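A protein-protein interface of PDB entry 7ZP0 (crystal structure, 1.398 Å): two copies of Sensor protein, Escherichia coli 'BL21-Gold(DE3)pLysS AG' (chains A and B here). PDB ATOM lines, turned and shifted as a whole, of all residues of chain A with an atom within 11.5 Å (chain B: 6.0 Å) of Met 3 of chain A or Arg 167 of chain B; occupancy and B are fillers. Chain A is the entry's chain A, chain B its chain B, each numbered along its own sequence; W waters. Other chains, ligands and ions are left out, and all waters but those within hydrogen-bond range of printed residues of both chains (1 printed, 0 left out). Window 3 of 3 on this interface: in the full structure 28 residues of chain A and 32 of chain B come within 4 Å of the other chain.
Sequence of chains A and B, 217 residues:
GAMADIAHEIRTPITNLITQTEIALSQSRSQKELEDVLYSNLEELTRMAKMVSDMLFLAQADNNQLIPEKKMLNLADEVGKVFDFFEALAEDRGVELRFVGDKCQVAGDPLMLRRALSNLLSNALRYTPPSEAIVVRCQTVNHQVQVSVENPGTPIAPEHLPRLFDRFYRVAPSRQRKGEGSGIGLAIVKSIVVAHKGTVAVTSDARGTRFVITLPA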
ATOM      1  N   GLY A   1       9.216  25.464  12.435  1.00  0.00           N
ATOM      2  CA  GLY A   1       9.330  25.852  13.828  1.00  0.00           C
ATOM      3  C   GLY A   1      10.045  27.179  13.994  1.00  0.00           C
ATOM      4  O   GLY A   1      10.558  27.749  13.028  1.00  0.00           O
ATOM      5  N   ALA A   2      10.093  27.660  15.231  1.00  0.00           N
ATOM      6  CA  ALA A   2      10.635  28.982  15.527  1.00  0.00           C
ATOM      7  C   ALA A   2      12.095  29.160  15.087  1.00  0.00           C
ATOM      8  O   ALA A   2      12.417  30.147  14.423  1.00  0.00           O
ATOM      9  CB  ALA A   2      10.488  29.278  17.016  1.00  0.00           C
ATOM     10  N   MET A   3      12.956  28.214  15.463  1.00  0.00           N
ATOM     11  CA  MET A   3      14.377  28.295  15.145  1.00  0.00           C
ATOM     12  C   MET A   3      14.620  28.233  13.640  1.00  0.00           C
ATOM     13  O   MET A   3      15.395  29.034  13.095  1.00  0.00           O
ATOM     14  CB  MET A   3      15.155  27.183  15.843  1.00  0.00           C
ATOM     15  CG  MET A   3      16.637  27.201  15.510  1.00  0.00           C
ATOM     16  SD  MET A   3      17.603  26.062  16.505  1.00  0.00           S
ATOM     17  CE  MET A   3      16.858  24.512  16.005  1.00  0.00           C
ATOM     18  N   ALA A   4      13.954  27.295  12.968  1.00  0.00           N
ATOM     19  CA  ALA A   4      14.055  27.191  11.517  1.00  0.00           C
ATOM     20  C   ALA A   4      13.631  28.493  10.826  1.00  0.00           C
ATOM     21  O   ALA A   4      14.286  28.952   9.904  1.00  0.00           O
ATOM     22  CB  ALA A   4      13.220  26.027  11.012  1.00  0.00           C
ATOM     23  N   ASP A   5      12.541  29.098  11.276  1.00  0.00           N
ATOM     24  CA  ASP A   5      12.084  30.348  10.667  1.00  0.00           C
ATOM     25  C   ASP A   5      13.132  31.446  10.788  1.00  0.00           C
ATOM     26  O   ASP A   5      13.400  32.163   9.824  1.00  0.00           O
ATOM     27  CB  ASP A   5      10.773  30.833  11.297  1.00  0.00           C
ATOM     28  CG  ASP A   5       9.571  29.978  10.902  1.00  0.00           C
ATOM     29  OD1 ASP A   5       9.685  29.206   9.926  1.00  0.00           O
ATOM     30  OD2 ASP A   5       8.505  30.116  11.543  1.00  0.00           O
ATOM     31  N   ILE A   6      13.731  31.570  11.970  1.00  0.00           N
ATOM     32  CA  ILE A   6      14.713  32.625  12.196  1.00  0.00           C
ATOM     33  C   ILE A   6      15.973  32.334  11.390  1.00  0.00           C
ATOM     34  O   ILE A   6      16.545  33.234  10.781  1.00  0.00           O
ATOM     35  CB  ILE A   6      15.058  32.772  13.692  1.00  0.00           C
ATOM     36  CG1 ILE A   6      13.817  33.216  14.477  1.00  0.00           C
ATOM     37  CG2 ILE A   6      16.218  33.762  13.895  1.00  0.00           C
ATOM     38  CD1 ILE A   6      13.909  32.908  15.947  1.00  0.00           C
ATOM     39  N   ALA A   7      16.395  31.069  11.382  1.00  0.00           N
ATOM     40  CA  ALA A   7      17.556  30.640  10.599  1.00  0.00           C
ATOM     41  C   ALA A   7      17.409  30.996   9.118  1.00  0.00           C
ATOM     42  O   ALA A   7      18.336  31.527   8.498  1.00  0.00           O
ATOM     43  CB  ALA A   7      17.778  29.135  10.764  1.00  0.00           C
ATOM     44  N   HIS A   8      16.240  30.718   8.550  1.00  0.00           N
ATOM     45  CA  HIS A   8      16.005  31.041   7.145  1.00  0.00           C
ATOM     46  C   HIS A   8      16.031  32.545   6.885  1.00  0.00           C
ATOM     47  O   HIS A   8      16.501  32.990   5.837  1.00  0.00           O
ATOM     48  CB  HIS A   8      14.677  30.448   6.663  1.00  0.00           C
ATOM     49  CG  HIS A   8      14.722  28.966   6.451  1.00  0.00           C
ATOM     50  ND1 HIS A   8      15.655  28.362   5.634  1.00  0.00           N
ATOM     51  CD2 HIS A   8      13.937  27.970   6.925  1.00  0.00           C
ATOM     52  CE1 HIS A   8      15.454  27.057   5.632  1.00  0.00           C
ATOM     53  NE2 HIS A   8      14.418  26.791   6.405  1.00  0.00           N
ATOM     54  N   GLU A   9      15.545  33.332   7.839  1.00  0.00           N
ATOM     55  CA  GLU A   9      15.484  34.773   7.639  1.00  0.00           C
ATOM     56  C   GLU A   9      16.874  35.407   7.659  1.00  0.00           C
ATOM     57  O   GLU A   9      17.196  36.235   6.816  1.00  0.00           O
ATOM     58  CB  GLU A   9      14.599  35.431   8.699  1.00  0.00           C
ATOM     59  CG  GLU A   9      14.176  36.847   8.342  1.00  0.00           C
ATOM     60  CD  GLU A   9      13.149  36.897   7.216  1.00  0.00           C
ATOM     61  OE1 GLU A   9      12.410  35.907   7.022  1.00  0.00           O
ATOM     62  OE2 GLU A   9      13.087  37.929   6.517  1.00  0.00           O
ATOM     63  N   ILE A  10      17.707  35.018   8.617  1.00  0.00           N
ATOM     64  CA  ILE A  10      19.015  35.651   8.735  1.00  0.00           C
ATOM     65  C   ILE A  10      20.022  35.091   7.743  1.00  0.00           C
ATOM     66  O   ILE A  10      21.060  35.706   7.506  1.00  0.00           O
ATOM     67  CB  ILE A  10      19.600  35.502  10.145  1.00  0.00           C
ATOM     68  CG1 ILE A  10      19.955  34.040  10.404  1.00  0.00           C
ATOM     69  CG2 ILE A  10      18.642  36.062  11.187  1.00  0.00           C
ATOM     70  CD1 ILE A  10      20.513  33.789  11.766  1.00  0.00           C
ATOM     71  N   ARG A  11      19.718  33.937   7.159  1.00  0.00           N
ATOM     72  CA  ARG A  11      20.662  33.298   6.244  1.00  0.00           C
ATOM     73  C   ARG A  11      20.973  34.185   5.041  1.00  0.00           C
ATOM     74  O   ARG A  11      22.141  34.378   4.692  1.00  0.00           O
ATOM     75  CB  ARG A  11      20.122  31.946   5.772  1.00  0.00           C
ATOM     76  CG  ARG A  11      21.025  31.275   4.755  1.00  0.00           C
ATOM     77  CD  ARG A  11      20.630  29.833   4.521  1.00  0.00           C
ATOM     78  NE  ARG A  11      19.302  29.715   3.927  1.00  0.00           N
ATOM     79  CZ  ARG A  11      18.660  28.562   3.760  1.00  0.00           C
ATOM     80  NH1 ARG A  11      17.452  28.546   3.212  1.00  0.00           N
ATOM     81  NH2 ARG A  11      19.225  27.425   4.142  1.00  0.00           N
ATOM     82  N   THR A  12      19.938  34.739   4.415  1.00  0.00           N
ATOM     83  CA  THR A  12      20.124  35.494   3.171  1.00  0.00           C
ATOM     84  C   THR A  12      21.094  36.684   3.311  1.00  0.00           C
ATOM     85  O   THR A  12      22.022  36.801   2.511  1.00  0.00           O
ATOM     86  CB  THR A  12      18.771  35.994   2.606  1.00  0.00           C
ATOM     87  OG1 THR A  12      17.762  35.009   2.833  1.00  0.00           O
ATOM     88  CG2 THR A  12      18.883  36.265   1.114  1.00  0.00           C
ATOM     89  N   ILE A  14      23.481  37.127   5.552  1.00  0.00           N
ATOM     90  CA  ILE A  14      24.794  36.550   5.834  1.00  0.00           C
ATOM     91  C   ILE A  14      25.430  36.055   4.544  1.00  0.00           C
ATOM     92  O   ILE A  14      26.586  36.364   4.240  1.00  0.00           O
ATOM     93  CB  ILE A  14      24.693  35.387   6.837  1.00  0.00           C
ATOM     94  CG1 ILE A  14      24.215  35.914   8.185  1.00  0.00           C
ATOM     95  CG2 ILE A  14      26.057  34.697   6.997  1.00  0.00           C
ATOM     96  CD1 ILE A  14      23.984  34.831   9.219  1.00  0.00           C
ATOM     97  N   MET A  51      17.628  44.313  11.985  1.00  0.00           N
ATOM     98  CA  MET A  51      16.959  43.020  12.069  1.00  0.00           C
ATOM     99  C   MET A  51      17.056  42.381  13.461  1.00  0.00           C
ATOM    100  O   MET A  51      16.051  41.932  14.017  1.00  0.00           O
ATOM    101  CB  MET A  51      17.547  42.074  11.021  1.00  0.00           C
ATOM    102  CG  MET A  51      17.067  40.640  11.090  1.00  0.00           C
ATOM    103  SD  MET A  51      17.859  39.639   9.807  1.00  0.00           S
ATOM    104  CE  MET A  51      19.591  39.825  10.230  1.00  0.00           C
ATOM    105  N   MET A  55      14.252  41.634  16.402  1.00  0.00           N
ATOM    106  CA  MET A  55      14.096  40.329  17.039  1.00  0.00           C
ATOM    107  C   MET A  55      14.092  40.437  18.559  1.00  0.00           C
ATOM    108  O   MET A  55      13.270  39.817  19.233  1.00  0.00           O
ATOM    109  CB  MET A  55      15.218  39.387  16.601  1.00  0.00           C
ATOM    110  CG  MET A  55      15.211  39.056  15.123  1.00  0.00           C
ATOM    111  SD  MET A  55      16.696  38.123  14.690  1.00  0.00           S
ATOM    112  CE  MET A  55      16.610  36.790  15.886  1.00  0.00           C
ATOM    113  N   ASP A  62       7.329  38.771  23.725  1.00  0.00           N
ATOM    114  CA  ASP A  62       7.114  37.352  23.996  1.00  0.00           C
ATOM    115  C   ASP A  62       7.230  37.031  25.484  1.00  0.00           C
ATOM    116  O   ASP A  62       6.482  36.216  26.010  1.00  0.00           O
ATOM    117  CB  ASP A  62       8.123  36.507  23.221  1.00  0.00           C
ATOM    118  CG  ASP A  62       7.834  36.455  21.732  1.00  0.00           C
ATOM    119  OD1 ASP A  62       6.817  37.038  21.280  1.00  0.00           O
ATOM    120  OD2 ASP A  62       8.655  35.846  21.014  1.00  0.00           O
ATOM    121  N   ARG A 167       4.676  35.864  12.840  1.00  0.00           N
ATOM    122  CA  ARG A 167       6.082  36.086  12.529  1.00  0.00           C
ATOM    123  C   ARG A 167       6.534  35.188  11.376  1.00  0.00           C
ATOM    124  O   ARG A 167       6.206  33.993  11.329  1.00  0.00           O
ATOM    125  CB  ARG A 167       6.946  35.862  13.778  1.00  0.00           C
ATOM    126  CG  ARG A 167       6.859  34.469  14.391  1.00  0.00           C
ATOM    127  CD  ARG A 167       7.454  34.457  15.788  1.00  0.00           C
ATOM    128  NE  ARG A 167       6.682  35.318  16.676  1.00  0.00           N
ATOM    129  CZ  ARG A 167       7.034  35.640  17.913  1.00  0.00           C
ATOM    130  NH1 ARG A 167       8.181  35.198  18.422  1.00  0.00           N
ATOM    131  NH2 ARG A 167       6.253  36.433  18.628  1.00  0.00           N
ATOM    132  N   PHE A 168       7.232  35.803  10.421  1.00  0.00           N
ATOM    133  CA  PHE A 168       7.820  35.115   9.260  1.00  0.00           C
ATOM    134  C   PHE A 168       6.797  34.485   8.306  1.00  0.00           C
ATOM    135  O   PHE A 168       7.176  33.740   7.387  1.00  0.00           O
ATOM    136  CB  PHE A 168       8.823  34.055   9.727  1.00  0.00           C
ATOM    137  CG  PHE A 168       9.884  34.607  10.632  1.00  0.00           C
ATOM    138  CD1 PHE A 168      10.784  35.546  10.165  1.00  0.00           C
ATOM    139  CD2 PHE A 168       9.965  34.215  11.959  1.00  0.00           C
ATOM    140  CE1 PHE A 168      11.753  36.072  10.988  1.00  0.00           C
ATOM    141  CE2 PHE A 168      10.939  34.737  12.792  1.00  0.00           C
ATOM    142  CZ  PHE A 168      11.828  35.670  12.305  1.00  0.00           C
ATOM    143  N   ILE A 184       9.178  40.116  10.509  1.00  0.00           N
ATOM    144  CA  ILE A 184       8.451  40.251  11.768  1.00  0.00           C
ATOM    145  C   ILE A 184       7.866  41.642  12.006  1.00  0.00           C
ATOM    146  O   ILE A 184       7.414  41.928  13.111  1.00  0.00           O
ATOM    147  CB  ILE A 184       9.340  39.883  12.978  1.00  0.00           C
ATOM    148  CG1 ILE A 184      10.571  40.789  13.079  1.00  0.00           C
ATOM    149  CG2 ILE A 184       9.734  38.413  12.926  1.00  0.00           C
ATOM    150  CD1 ILE A 184      11.432  40.484  14.305  1.00  0.00           C
ATOM    151  N   ALA B   2      13.953  30.744  21.253  1.00  0.00           N
ATOM    152  CA  ALA B   2      14.873  30.878  20.126  1.00  0.00           C
ATOM    153  C   ALA B   2      15.067  32.326  19.676  1.00  0.00           C
ATOM    154  O   ALA B   2      16.162  32.716  19.278  1.00  0.00           O
ATOM    155  CB  ALA B   2      14.384  30.039  18.958  1.00  0.00           C
ATOM    156  N   ASP B   5      17.438  33.854  22.116  1.00  0.00           N
ATOM    157  CA  ASP B   5      18.702  33.114  22.128  1.00  0.00           C
ATOM    158  C   ASP B   5      19.538  33.361  20.874  1.00  0.00           C
ATOM    159  O   ASP B   5      20.752  33.583  20.947  1.00  0.00           O
ATOM    160  CB  ASP B   5      18.443  31.611  22.274  1.00  0.00           C
ATOM    161  CG  ASP B   5      18.043  31.215  23.685  1.00  0.00           C
ATOM    162  OD1 ASP B   5      18.150  32.051  24.605  1.00  0.00           O
ATOM    163  OD2 ASP B   5      17.623  30.054  23.869  1.00  0.00           O
ATOM    164  N   ILE B   6      18.887  33.308  19.718  1.00  0.00           N
ATOM    165  CA  ILE B   6      19.582  33.528  18.457  1.00  0.00           C
ATOM    166  C   ILE B   6      19.992  34.985  18.295  1.00  0.00           C
ATOM    167  O   ILE B   6      21.102  35.278  17.854  1.00  0.00           O
ATOM    168  CB  ILE B   6      18.707  33.085  17.273  1.00  0.00           C
ATOM    169  CG1 ILE B   6      18.448  31.583  17.380  1.00  0.00           C
ATOM    170  CG2 ILE B   6      19.356  33.436  15.943  1.00  0.00           C
ATOM    171  CD1 ILE B   6      17.372  31.082  16.459  1.00  0.00           C
ATOM    172  N   ASP B  54      23.983  24.817  11.468  1.00  0.00           N
ATOM    173  CA  ASP B  54      23.715  23.993  12.640  1.00  0.00           C
ATOM    174  C   ASP B  54      22.242  24.098  13.058  1.00  0.00           C
ATOM    175  O   ASP B  54      21.609  23.092  13.385  1.00  0.00           O
ATOM    176  CB  ASP B  54      24.646  24.387  13.802  1.00  0.00           C
ATOM    177  CG  ASP B  54      25.973  23.629  13.790  1.00  0.00           C
ATOM    178  OD1 ASP B  54      26.237  22.859  12.838  1.00  0.00           O
ATOM    179  OD2 ASP B  54      26.769  23.814  14.746  1.00  0.00           O
ATOM    180  N   MET B  55      21.690  25.305  13.038  1.00  0.00           N
ATOM    181  CA  MET B  55      20.298  25.489  13.464  1.00  0.00           C
ATOM    182  C   MET B  55      19.310  24.736  12.584  1.00  0.00           C
ATOM    183  O   MET B  55      18.336  24.163  13.097  1.00  0.00           O
ATOM    184  CB  MET B  55      19.932  26.973  13.506  1.00  0.00           C
ATOM    185  CG  MET B  55      20.591  27.690  14.667  1.00  0.00           C
ATOM    186  SD  MET B  55      19.964  29.352  14.898  1.00  0.00           S
ATOM    187  CE  MET B  55      20.539  30.099  13.384  1.00  0.00           C
ATOM    188  N   LEU B  56      19.566  24.721  11.278  1.00  0.00           N
ATOM    189  CA  LEU B  56      18.679  24.024  10.355  1.00  0.00           C
ATOM    190  C   LEU B  56      18.773  22.512  10.549  1.00  0.00           C
ATOM    191  O   LEU B  56      17.775  21.806  10.402  1.00  0.00           O
ATOM    192  CB  LEU B  56      18.983  24.420   8.906  1.00  0.00           C
ATOM    193  CG  LEU B  56      18.559  25.861   8.627  1.00  0.00           C
ATOM    194  CD1 LEU B  56      19.131  26.356   7.302  1.00  0.00           C
ATOM    195  CD2 LEU B  56      17.024  25.977   8.658  1.00  0.00           C
ATOM    196  N   LEU B  58      19.490  20.984  13.505  1.00  0.00           N
ATOM    197  CA  LEU B  58      18.830  20.722  14.770  1.00  0.00           C
ATOM    198  C   LEU B  58      17.321  20.860  14.623  1.00  0.00           C
ATOM    199  O   LEU B  58      16.565  20.146  15.281  1.00  0.00           O
ATOM    200  CB  LEU B  58      19.356  21.674  15.842  1.00  0.00           C
ATOM    201  CG  LEU B  58      18.875  21.448  17.275  1.00  0.00           C
ATOM    202  CD1 LEU B  58      19.125  20.005  17.696  1.00  0.00           C
ATOM    203  CD2 LEU B  58      19.563  22.422  18.223  1.00  0.00           C
ATOM    204  N   ALA B  59      16.881  21.761  13.746  1.00  0.00           N
ATOM    205  CA  ALA B  59      15.451  21.988  13.561  1.00  0.00           C
ATOM    206  C   ALA B  59      14.740  20.732  13.077  1.00  0.00           C
ATOM    207  O   ALA B  59      13.573  20.554  13.373  1.00  0.00           O
ATOM    208  CB  ALA B  59      15.205  23.148  12.591  1.00  0.00           C
ATOM    209  N   ALA B  61      15.219  17.769  14.155  1.00  0.00           N
ATOM    210  CA  ALA B  61      14.955  16.990  15.361  1.00  0.00           C
ATOM    211  C   ALA B  61      13.661  17.419  16.035  1.00  0.00           C
ATOM    212  O   ALA B  61      12.841  16.582  16.410  1.00  0.00           O
ATOM    213  CB  ALA B  61      16.100  17.126  16.317  1.00  0.00           C
ATOM    214  N   ASP B  62      13.493  18.728  16.210  1.00  0.00           N
ATOM    215  CA  ASP B  62      12.176  19.290  16.482  1.00  0.00           C
ATOM    216  C   ASP B  62      11.381  18.956  15.236  1.00  0.00           C
ATOM    217  O   ASP B  62      11.981  18.756  14.198  1.00  0.00           O
ATOM    218  CB  ASP B  62      12.238  20.798  16.727  1.00  0.00           C
ATOM    219  CG  ASP B  62      13.438  21.206  17.558  1.00  0.00           C
ATOM    220  OD1 ASP B  62      14.023  20.336  18.237  1.00  0.00           O
ATOM    221  OD2 ASP B  62      13.806  22.400  17.528  1.00  0.00           O
ATOM    222  N   ARG B 163      23.476  20.993  32.073  1.00  0.00           N
ATOM    223  CA  ARG B 163      23.117  22.051  31.130  1.00  0.00           C
ATOM    224  C   ARG B 163      23.894  22.003  29.818  1.00  0.00           C
ATOM    225  O   ARG B 163      23.561  22.724  28.881  1.00  0.00           O
ATOM    226  CB  ARG B 163      23.349  23.428  31.766  1.00  0.00           C
ATOM    227  CG  ARG B 163      22.544  23.722  32.998  1.00  0.00           C
ATOM    228  CD  ARG B 163      21.094  23.989  32.670  1.00  0.00           C
ATOM    229  NE  ARG B 163      20.311  22.760  32.710  1.00  0.00           N
ATOM    230  CZ  ARG B 163      19.847  22.195  33.823  1.00  0.00           C
ATOM    231  NH1 ARG B 163      19.147  21.069  33.745  1.00  0.00           N
ATOM    232  NH2 ARG B 163      20.070  22.756  35.008  1.00  0.00           N
ATOM    233  N   PHE B 165      24.242  20.233  27.213  1.00  0.00           N
ATOM    234  CA  PHE B 165      23.650  19.903  25.926  1.00  0.00           C
ATOM    235  C   PHE B 165      22.488  20.826  25.580  1.00  0.00           C
ATOM    236  O   PHE B 165      21.840  20.634  24.569  1.00  0.00           O
ATOM    237  CB  PHE B 165      23.184  18.441  25.911  1.00  0.00           C
ATOM    238  CG  PHE B 165      24.269  17.465  26.248  1.00  0.00           C
ATOM    239  CD1 PHE B 165      25.137  17.020  25.274  1.00  0.00           C
ATOM    240  CD2 PHE B 165      24.444  17.020  27.544  1.00  0.00           C
ATOM    241  CE1 PHE B 165      26.154  16.140  25.582  1.00  0.00           C
ATOM    242  CE2 PHE B 165      25.460  16.143  27.858  1.00  0.00           C
ATOM    243  CZ  PHE B 165      26.317  15.698  26.871  1.00  0.00           C
ATOM    244  N   ASP B 166      22.229  21.822  26.417  1.00  0.00           N
ATOM    245  CA  ASP B 166      21.172  22.780  26.124  1.00  0.00           C
ATOM    246  C   ASP B 166      21.579  23.691  24.967  1.00  0.00           C
ATOM    247  O   ASP B 166      22.736  24.089  24.869  1.00  0.00           O
ATOM    248  CB  ASP B 166      20.841  23.636  27.355  1.00  0.00           C
ATOM    249  CG  ASP B 166      20.170  22.848  28.469  1.00  0.00           C
ATOM    250  OD1 ASP B 166      19.915  21.639  28.298  1.00  0.00           O
ATOM    251  OD2 ASP B 166      19.885  23.461  29.521  1.00  0.00           O
ATOM    252  N   ARG B 167      20.628  24.030  24.104  1.00  0.00           N
ATOM    253  CA  ARG B 167      20.869  24.989  23.030  1.00  0.00           C
ATOM    254  C   ARG B 167      21.400  26.303  23.569  1.00  0.00           C
ATOM    255  O   ARG B 167      20.796  26.907  24.465  1.00  0.00           O
ATOM    256  CB  ARG B 167      19.588  25.263  22.247  1.00  0.00           C
ATOM    257  CG  ARG B 167      19.019  24.070  21.531  1.00  0.00           C
ATOM    258  CD  ARG B 167      17.512  24.208  21.295  1.00  0.00           C
ATOM    259  NE  ARG B 167      16.987  22.941  20.805  1.00  0.00           N
ATOM    260  CZ  ARG B 167      16.210  22.794  19.741  1.00  0.00           C
ATOM    261  NH1 ARG B 167      15.810  23.849  19.050  1.00  0.00           N
ATOM    262  NH2 ARG B 167      15.811  21.581  19.389  1.00  0.00           N
ATOM    263  N   PHE B 168      22.535  26.719  23.025  1.00  0.00           N
ATOM    264  CA  PHE B 168      23.143  28.011  23.318  1.00  0.00           C
ATOM    265  C   PHE B 168      23.558  28.197  24.773  1.00  0.00           C
ATOM    266  O   PHE B 168      23.786  29.324  25.202  1.00  0.00           O
ATOM    267  CB  PHE B 168      22.203  29.139  22.887  1.00  0.00           C
ATOM    268  CG  PHE B 168      21.830  29.075  21.438  1.00  0.00           C
ATOM    269  CD1 PHE B 168      22.759  29.394  20.463  1.00  0.00           C
ATOM    270  CD2 PHE B 168      20.554  28.697  21.045  1.00  0.00           C
ATOM    271  CE1 PHE B 168      22.427  29.335  19.122  1.00  0.00           C
ATOM    272  CE2 PHE B 168      20.217  28.633  19.704  1.00  0.00           C
ATOM    273  CZ  PHE B 168      21.153  28.957  18.742  1.00  0.00           C
ATOM    274  N   TYR B 169      23.678  27.105  25.529  1.00  0.00           N
ATOM    275  CA  TYR B 169      24.274  27.193  26.858  1.00  0.00           C
ATOM    276  C   TYR B 169      25.792  27.259  26.760  1.00  0.00           C
ATOM    277  O   TYR B 169      26.412  26.469  26.051  1.00  0.00           O
ATOM    278  CB  TYR B 169      23.872  26.007  27.733  1.00  0.00           C
ATOM    279  CG  TYR B 169      24.345  26.171  29.157  1.00  0.00           C
ATOM    280  CD1 TYR B 169      23.614  26.932  30.059  1.00  0.00           C
ATOM    281  CD2 TYR B 169      25.535  25.599  29.591  1.00  0.00           C
ATOM    282  CE1 TYR B 169      24.033  27.099  31.362  1.00  0.00           C
ATOM    283  CE2 TYR B 169      25.968  25.768  30.894  1.00  0.00           C
ATOM    284  CZ  TYR B 169      25.217  26.519  31.772  1.00  0.00           C
ATOM    285  OH  TYR B 169      25.645  26.688  33.065  1.00  0.00           O
ATOM    286  N   GLY B 183      27.280  27.231  19.339  1.00  0.00           N
ATOM    287  CA  GLY B 183      26.447  27.351  20.512  1.00  0.00           C
ATOM    288  C   GLY B 183      25.466  26.200  20.614  1.00  0.00           C
ATOM    289  O   GLY B 183      24.846  26.016  21.663  1.00  0.00           O
ATOM    290  N   ILE B 184      25.312  25.418  19.541  1.00  0.00           N
ATOM    291  CA  ILE B 184      24.412  24.263  19.589  1.00  0.00           C
ATOM    292  C   ILE B 184      25.093  22.960  19.150  1.00  0.00           C
ATOM    293  O   ILE B 184      24.431  21.965  18.847  1.00  0.00           O
ATOM    294  CB  ILE B 184      23.130  24.498  18.746  1.00  0.00           C
ATOM    295  CG1 ILE B 184      23.465  24.918  17.316  1.00  0.00           C
ATOM    296  CG2 ILE B 184      22.258  25.549  19.410  1.00  0.00           C
ATOM    297  CD1 ILE B 184      22.263  24.876  16.394  1.00  0.00           C
ATOM    298  N   ALA B 187      24.060  20.323  21.738  1.00  0.00           N
ATOM    299  CA  ALA B 187      22.649  20.013  21.554  1.00  0.00           C
ATOM    300  C   ALA B 187      22.485  19.102  20.342  1.00  0.00           C
ATOM    301  O   ALA B 187      21.668  18.168  20.355  1.00  0.00           O
ATOM    302  CB  ALA B 187      21.834  21.278  21.395  1.00  0.00           C
HETATM  303  O   HOH W   1      11.852  23.223  12.183  1.00  0.00           O
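The side-chain carboxylate (OD1) of Asp 62 of chain B is in salt-bridge range of the guanidinium group (NH2) of Arg 167 of chain B (2.5 Å). ND1 of His 8 of chain A is in hydrogen-bond range of NH1 of Arg 11 of chain A, at 3.0 Å.
Among the printed residues, merely in contact across the chains: Met 3 of chain A with Met 55 of chain B, Met 3 of chain A with Arg 167 of chain B, Arg 11 of chain A with Leu 56 of chain B, His 8 of chain A with Leu 56 of chain B, Met 3 of chain A with Ala 59 of chain B, Ile 6 of chain A with Ile 6 of chain B, Met 3 of chain A with Leu 58 of chain B, Ala 4 of chain A with Ala 59 of chain B, Ala 7 of chain A with Leu 56 of chain B, Ala 7 of chain A with Met 55 of chain B and Ile 6 of chain A with Ala 2 of chain B.
Of the printed residues of chain B, Met 3 of chain A touches Met 55 (3.3 Å), Leu 58 (3.8 Å), Ala 59 (3.6 Å) and Arg 167 (3.3 Å). Arg 167 of chain B touches one residue of chain A. Of the printed residues of chain A, Met 55 of chain B touches Met 3 and Ala 7. Leu 56 of chain B touches just these residues of chain A: Ala 7, His 8 and Arg 11. Of chain A, only Met 3 (3.8 Å) comes within 4 Å of Leu 58 of chain B. No residue of chain A comes within 4 Å of Ala 61 of chain B. No residue of chain A comes within 4 Å of Phe 168 of chain B. No residue of chain A comes within 4 Å of Gly 183 of chain B. No residue of chain A comes within 4 Å of Ile 184 of chain B. Printed residues of chain B within 4 Å of Ile 6 of chain A: Ala 2 and Ile 6. Printed residues of chain B within 4 Å of Ala 7 of chain A: Met 55 and Leu 56. Printed residues of chain A within 4 Å of Ile 6 of chain B: Ile 6 (3.8 Å). Ala 2 of chain A touches none of the printed residues of chain B. Glu 9 of chain A touches none of the printed residues of chain B.
Printed residues of chain B that touch a printed residue of chain A: Ala 2, Ile 6, Met 55, Leu 56, Leu 58, Ala 59 and Arg 167. Hydrophobic or aromatic side chains of chain A that line the printed part of chain B: Met 3, Ala 4, Ile 6, Ala 7 and His 8. Along chain A the printed residues that touch a printed residue of chain B span positions 3 to 11. Among the printed residues, 11 pairs touch across the chains. Among the printed residues, no Asp or Glu carboxylate lies within 4 Å of a Lys or Arg side-chain nitrogen of the other chain.
Ile 6 of chain A touches Ala 2 of chain B, but with the chains exchanged Ala 2 of chain A does not touch Ile 6 of chain B (5.4 Å). Ile 6 of chain B touches its own counterpart, Ile 6 of chain A. 8 positions are printed for both chains. Of the 11 pairs that touch across the chains among the printed residues, 1 has its exchanged pair printed and touching as well.
Water W1 bridges the backbone carbonyl oxygen of Ala 59 of chain B (3.4 Å) and the backbone NH of Gly 1 of chain A (3.5 Å).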
